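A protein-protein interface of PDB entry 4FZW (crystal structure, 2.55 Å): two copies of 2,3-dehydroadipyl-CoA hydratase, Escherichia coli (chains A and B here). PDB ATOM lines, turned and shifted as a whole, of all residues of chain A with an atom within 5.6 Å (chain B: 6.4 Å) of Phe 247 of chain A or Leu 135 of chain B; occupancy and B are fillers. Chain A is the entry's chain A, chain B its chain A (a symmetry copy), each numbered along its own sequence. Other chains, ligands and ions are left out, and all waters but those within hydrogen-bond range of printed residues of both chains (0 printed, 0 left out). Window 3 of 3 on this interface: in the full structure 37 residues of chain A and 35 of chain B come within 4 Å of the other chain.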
ATOM      1  N   ASP A 239     -11.881 -17.892  -6.005  1.00  0.00           N
ATOM      2  CA  ASP A 239     -11.474 -16.886  -6.980  1.00  0.00           C
ATOM      3  C   ASP A 239     -10.222 -16.127  -6.544  1.00  0.00           C
ATOM      4  O   ASP A 239      -9.474 -15.648  -7.372  1.00  0.00           O
ATOM      5  CB  ASP A 239     -12.620 -15.917  -7.277  1.00  0.00           C
ATOM      6  CG  ASP A 239     -13.762 -16.578  -8.041  1.00  0.00           C
ATOM      7  OD1 ASP A 239     -13.481 -17.486  -8.853  1.00  0.00           O
ATOM      8  OD2 ASP A 239     -14.936 -16.194  -7.828  1.00  0.00           O
ATOM      9  N   ARG A 240      -9.985 -16.021  -5.243  1.00  0.00           N
ATOM     10  CA  ARG A 240      -8.746 -15.417  -4.770  1.00  0.00           C
ATOM     11  C   ARG A 240      -7.576 -16.171  -5.378  1.00  0.00           C
ATOM     12  O   ARG A 240      -6.635 -15.565  -5.900  1.00  0.00           O
ATOM     13  CB  ARG A 240      -8.668 -15.475  -3.249  1.00  0.00           C
ATOM     14  CG  ARG A 240      -7.415 -14.877  -2.669  1.00  0.00           C
ATOM     15  CD  ARG A 240      -7.497 -14.950  -1.153  1.00  0.00           C
ATOM     16  NE  ARG A 240      -6.369 -14.329  -0.470  1.00  0.00           N
ATOM     17  CZ  ARG A 240      -5.277 -14.981  -0.084  1.00  0.00           C
ATOM     18  NH1 ARG A 240      -5.163 -16.283  -0.308  1.00  0.00           N
ATOM     19  NH2 ARG A 240      -4.296 -14.326   0.524  1.00  0.00           N
ATOM     20  N   GLU A 242      -7.746 -18.030  -8.128  1.00  0.00           N
ATOM     21  CA  GLU A 242      -7.809 -17.803  -9.572  1.00  0.00           C
ATOM     22  C   GLU A 242      -7.278 -16.423  -9.963  1.00  0.00           C
ATOM     23  O   GLU A 242      -6.484 -16.294 -10.891  1.00  0.00           O
ATOM     24  CB  GLU A 242      -9.242 -17.987 -10.090  1.00  0.00           C
ATOM     25  CG  GLU A 242      -9.396 -17.778 -11.602  1.00  0.00           C
ATOM     26  CD  GLU A 242      -8.627 -18.805 -12.423  1.00  0.00           C
ATOM     27  OE1 GLU A 242      -8.181 -19.820 -11.847  1.00  0.00           O
ATOM     28  OE2 GLU A 242      -8.471 -18.602 -13.645  1.00  0.00           O
ATOM     29  N   GLY A 243      -7.726 -15.401  -9.244  1.00  0.00           N
ATOM     30  CA  GLY A 243      -7.311 -14.035  -9.486  1.00  0.00           C
ATOM     31  C   GLY A 243      -5.807 -13.819  -9.514  1.00  0.00           C
ATOM     32  O   GLY A 243      -5.312 -13.102 -10.382  1.00  0.00           O
ATOM     33  N   ILE A 244      -5.077 -14.418  -8.569  1.00  0.00           N
ATOM     34  CA  ILE A 244      -3.624 -14.213  -8.483  1.00  0.00           C
ATOM     35  C   ILE A 244      -2.824 -15.226  -9.305  1.00  0.00           C
ATOM     36  O   ILE A 244      -1.659 -14.981  -9.645  1.00  0.00           O
ATOM     37  CB  ILE A 244      -3.095 -14.245  -7.029  1.00  0.00           C
ATOM     38  CG1 ILE A 244      -3.315 -15.623  -6.412  1.00  0.00           C
ATOM     39  CG2 ILE A 244      -3.743 -13.157  -6.192  1.00  0.00           C
ATOM     40  CD1 ILE A 244      -2.350 -15.939  -5.298  1.00  0.00           C
ATOM     41  N   SER A 245      -3.444 -16.367  -9.598  1.00  0.00           N
ATOM     42  CA  SER A 245      -2.858 -17.353 -10.498  1.00  0.00           C
ATOM     43  C   SER A 245      -2.850 -16.774 -11.901  1.00  0.00           C
ATOM     44  O   SER A 245      -1.818 -16.724 -12.568  1.00  0.00           O
ATOM     45  CB  SER A 245      -3.687 -18.635 -10.491  1.00  0.00           C
ATOM     46  OG  SER A 245      -3.525 -19.340 -11.709  1.00  0.00           O
ATOM     47  N   ALA A 246      -4.026 -16.329 -12.331  1.00  0.00           N
ATOM     48  CA  ALA A 246      -4.194 -15.711 -13.629  1.00  0.00           C
ATOM     49  C   ALA A 246      -3.309 -14.479 -13.764  1.00  0.00           C
ATOM     50  O   ALA A 246      -2.949 -14.092 -14.870  1.00  0.00           O
ATOM     51  CB  ALA A 246      -5.652 -15.346 -13.844  1.00  0.00           C
ATOM     52  N   PHE A 247      -2.952 -13.869 -12.634  1.00  0.00           N
ATOM     53  CA  PHE A 247      -2.091 -12.686 -12.640  1.00  0.00           C
ATOM     54  C   PHE A 247      -0.611 -13.046 -12.687  1.00  0.00           C
ATOM     55  O   PHE A 247       0.168 -12.398 -13.385  1.00  0.00           O
ATOM     56  CB  PHE A 247      -2.365 -11.800 -11.422  1.00  0.00           C
ATOM     57  CG  PHE A 247      -1.365 -10.679 -11.242  1.00  0.00           C
ATOM     58  CD1 PHE A 247      -1.574  -9.435 -11.828  1.00  0.00           C
ATOM     59  CD2 PHE A 247      -0.218 -10.868 -10.482  1.00  0.00           C
ATOM     60  CE1 PHE A 247      -0.651  -8.399 -11.662  1.00  0.00           C
ATOM     61  CE2 PHE A 247       0.705  -9.841 -10.313  1.00  0.00           C
ATOM     62  CZ  PHE A 247       0.487  -8.605 -10.904  1.00  0.00           C
ATOM     63  N   LEU A 248      -0.226 -14.076 -11.937  1.00  0.00           N
ATOM     64  CA  LEU A 248       1.174 -14.487 -11.875  1.00  0.00           C
ATOM     65  C   LEU A 248       1.612 -15.232 -13.144  1.00  0.00           C
ATOM     66  O   LEU A 248       2.744 -15.074 -13.609  1.00  0.00           O
ATOM     67  CB  LEU A 248       1.448 -15.312 -10.612  1.00  0.00           C
ATOM     68  CG  LEU A 248       2.914 -15.659 -10.324  1.00  0.00           C
ATOM     69  CD1 LEU A 248       3.220 -15.643  -8.833  1.00  0.00           C
ATOM     70  CD2 LEU A 248       3.296 -16.999 -10.947  1.00  0.00           C
ATOM     71  N   GLN A 249       0.710 -16.031 -13.706  1.00  0.00           N
ATOM     72  CA  GLN A 249       0.969 -16.686 -14.988  1.00  0.00           C
ATOM     73  C   GLN A 249       0.315 -15.936 -16.148  1.00  0.00           C
ATOM     74  O   GLN A 249       0.060 -16.508 -17.209  1.00  0.00           O
ATOM     75  CB  GLN A 249       0.552 -18.160 -14.955  1.00  0.00           C
ATOM     76  CG  GLN A 249      -0.925 -18.412 -14.703  1.00  0.00           C
ATOM     77  CD  GLN A 249      -1.232 -19.884 -14.514  1.00  0.00           C
ATOM     78  OE1 GLN A 249      -1.064 -20.686 -15.427  1.00  0.00           O
ATOM     79  NE2 GLN A 249      -1.671 -20.249 -13.320  1.00  0.00           N
ATOM     80  N   LYS A 250       0.029 -14.655 -15.914  1.00  0.00           N
ATOM     81  CA  LYS A 250      -0.281 -13.675 -16.973  1.00  0.00           C
ATOM     82  C   LYS A 250      -1.385 -14.041 -17.973  1.00  0.00           C
ATOM     83  O   LYS A 250      -1.121 -14.176 -19.165  1.00  0.00           O
ATOM     84  CB  LYS A 250       0.994 -13.297 -17.729  1.00  0.00           C
ATOM     85  N   ARG A 251      -2.618 -14.163 -17.491  1.00  0.00           N
ATOM     86  CA  ARG A 251      -3.763 -14.402 -18.367  1.00  0.00           C
ATOM     87  C   ARG A 251      -4.977 -13.613 -17.882  1.00  0.00           C
ATOM     88  O   ARG A 251      -4.859 -12.755 -17.016  1.00  0.00           O
ATOM     89  CB  ARG A 251      -4.084 -15.900 -18.437  1.00  0.00           C
ATOM     90  CG  ARG A 251      -4.209 -16.566 -17.082  1.00  0.00           C
ATOM     91  CD  ARG A 251      -4.318 -18.082 -17.188  1.00  0.00           C
ATOM     92  NE  ARG A 251      -4.508 -18.687 -15.872  1.00  0.00           N
ATOM     93  CZ  ARG A 251      -5.671 -19.145 -15.420  1.00  0.00           C
ATOM     94  NH1 ARG A 251      -6.757 -19.094 -16.185  1.00  0.00           N
ATOM     95  NH2 ARG A 251      -5.748 -19.669 -14.201  1.00  0.00           N
ATOM     96  N   LEU B  68       3.929 -11.090  -2.672  1.00  0.00           N
ATOM     97  CA  LEU B  68       2.743 -11.799  -3.133  1.00  0.00           C
ATOM     98  C   LEU B  68       2.727 -13.271  -2.712  1.00  0.00           C
ATOM     99  O   LEU B  68       1.668 -13.900  -2.649  1.00  0.00           O
ATOM    100  CB  LEU B  68       2.624 -11.679  -4.656  1.00  0.00           C
ATOM    101  CG  LEU B  68       1.259 -12.043  -5.227  1.00  0.00           C
ATOM    102  CD1 LEU B  68       0.173 -11.285  -4.488  1.00  0.00           C
ATOM    103  CD2 LEU B  68       1.211 -11.751  -6.714  1.00  0.00           C
ATOM    104  N   PRO B 131      -4.404  -1.829  -6.384  1.00  0.00           N
ATOM    105  CA  PRO B 131      -4.767  -2.876  -7.352  1.00  0.00           C
ATOM    106  C   PRO B 131      -5.134  -4.211  -6.681  1.00  0.00           C
ATOM    107  O   PRO B 131      -5.142  -5.241  -7.347  1.00  0.00           O
ATOM    108  CB  PRO B 131      -3.492  -3.027  -8.187  1.00  0.00           C
ATOM    109  CG  PRO B 131      -2.374  -2.726  -7.194  1.00  0.00           C
ATOM    110  CD  PRO B 131      -2.940  -1.702  -6.208  1.00  0.00           C
ATOM    111  N   GLU B 132      -5.442  -4.203  -5.390  1.00  0.00           N
ATOM    112  CA  GLU B 132      -5.832  -5.460  -4.731  1.00  0.00           C
ATOM    113  C   GLU B 132      -6.959  -6.142  -5.488  1.00  0.00           C
ATOM    114  O   GLU B 132      -6.888  -7.318  -5.808  1.00  0.00           O
ATOM    115  CB  GLU B 132      -6.225  -5.246  -3.273  1.00  0.00           C
ATOM    116  CG  GLU B 132      -5.037  -5.003  -2.333  1.00  0.00           C
ATOM    117  CD  GLU B 132      -4.555  -3.565  -2.356  1.00  0.00           C
ATOM    118  OE1 GLU B 132      -5.146  -2.764  -3.111  1.00  0.00           O
ATOM    119  OE2 GLU B 132      -3.606  -3.228  -1.612  1.00  0.00           O
ATOM    120  N   ILE B 133      -7.981  -5.372  -5.820  1.00  0.00           N
ATOM    121  CA  ILE B 133      -9.143  -5.904  -6.512  1.00  0.00           C
ATOM    122  C   ILE B 133      -8.834  -6.699  -7.797  1.00  0.00           C
ATOM    123  O   ILE B 133      -9.580  -7.610  -8.126  1.00  0.00           O
ATOM    124  CB  ILE B 133     -10.175  -4.782  -6.807  1.00  0.00           C
ATOM    125  CG1 ILE B 133     -11.566  -5.377  -7.083  1.00  0.00           C
ATOM    126  CG2 ILE B 133      -9.675  -3.861  -7.940  1.00  0.00           C
ATOM    127  CD1 ILE B 133     -12.229  -5.940  -5.863  1.00  0.00           C
ATOM    128  N   THR B 134      -7.759  -6.368  -8.517  1.00  0.00           N
ATOM    129  CA  THR B 134      -7.433  -7.118  -9.735  1.00  0.00           C
ATOM    130  C   THR B 134      -6.906  -8.525  -9.436  1.00  0.00           C
ATOM    131  O   THR B 134      -6.906  -9.398 -10.317  1.00  0.00           O
ATOM    132  CB  THR B 134      -6.404  -6.403 -10.663  1.00  0.00           C
ATOM    133  OG1 THR B 134      -5.125  -6.343 -10.022  1.00  0.00           O
ATOM    134  CG2 THR B 134      -6.858  -4.996 -11.048  1.00  0.00           C
ATOM    135  N   LEU B 135      -6.449  -8.743  -8.205  1.00  0.00           N
ATOM    136  CA  LEU B 135      -5.845 -10.012  -7.850  1.00  0.00           C
ATOM    137  C   LEU B 135      -6.887 -10.956  -7.233  1.00  0.00           C
ATOM    138  O   LEU B 135      -6.574 -12.085  -6.847  1.00  0.00           O
ATOM    139  CB  LEU B 135      -4.677  -9.786  -6.888  1.00  0.00           C
ATOM    140  CG  LEU B 135      -3.508  -8.923  -7.371  1.00  0.00           C
ATOM    141  CD1 LEU B 135      -2.892  -8.141  -6.217  1.00  0.00           C
ATOM    142  CD2 LEU B 135      -2.465  -9.771  -8.069  1.00  0.00           C
ATOM    143  N   GLY B 136      -8.129 -10.496  -7.144  1.00  0.00           N
ATOM    144  CA  GLY B 136      -9.177 -11.272  -6.502  1.00  0.00           C
ATOM    145  C   GLY B 136      -9.148 -11.048  -5.000  1.00  0.00           C
ATOM    146  O   GLY B 136      -9.765 -11.794  -4.229  1.00  0.00           O
ATOM    147  N   ILE B 137      -8.412 -10.032  -4.570  1.00  0.00           N
ATOM    148  CA  ILE B 137      -8.486  -9.629  -3.179  1.00  0.00           C
ATOM    149  C   ILE B 137      -9.059  -8.220  -3.020  1.00  0.00           C
ATOM    150  O   ILE B 137      -9.941  -7.786  -3.771  1.00  0.00           O
ATOM    151  CB  ILE B 137      -7.117  -9.750  -2.466  1.00  0.00           C
ATOM    152  CG1 ILE B 137      -6.022  -8.979  -3.199  1.00  0.00           C
ATOM    153  CG2 ILE B 137      -6.668 -11.205  -2.372  1.00  0.00           C
ATOM    154  CD1 ILE B 137      -4.747  -8.851  -2.385  1.00  0.00           C
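Leu 135 of chain B touches just these residues of chain A: Arg 240 (3.6 Å), Gly 243 (3.3 Å), Ile 244 (3.1 Å) and Phe 247 (3.5 Å).
Of the printed residues of chain A, Ile 137 of chain B touches Arg 240.
Printed residues of chain A within 4 Å of Gly 136 of chain B: Arg 240.
Printed residues of chain B within 4 Å of Arg 240 of chain A: Leu 135 (3.6 Å), Gly 136 (3.8 Å) and Ile 137 (3.7 Å).
The nearest residue of chain A that does not touch Leu 135 of chain B is Asp 239 of chain A (4.6 Å).
The backbone carbonyl oxygen (O) of Glu 132 of chain B sits close to the backbone NH (N) of Ile 137 of chain B, at 3.3 Å.
Among the printed residues, merely in contact across the chains: Arg 240 of chain A with Leu 135 of chain B (3.6 Å), Arg 240 of chain A with Gly 136 of chain B (3.8 Å), Arg 240 of chain A with Ile 137 of chain B (3.7 Å), Gly 243 of chain A with Leu 135 of chain B (3.3 Å) and Phe 247 of chain A with Leu 135 of chain B (3.5 Å).
No position is printed for both chains.
Of the 6 pairs that touch across the chains among the printed residues, none has its exchanged pair printed and touching as well.
Of the 8 printed residues of chain B, 3 touch a printed residue of chain A.
Printed residues of chain B that touch a printed residue of chain A: Leu 135, Gly 136 and Ile 137.
Of the 12 printed residues of chain A, 4 touch a printed residue of chain B.
Among the printed residues, 6 pairs touch across the chains.
O of Leu 135 of chain B lies close to N of Ile 244 of chain A (3.3 Å).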
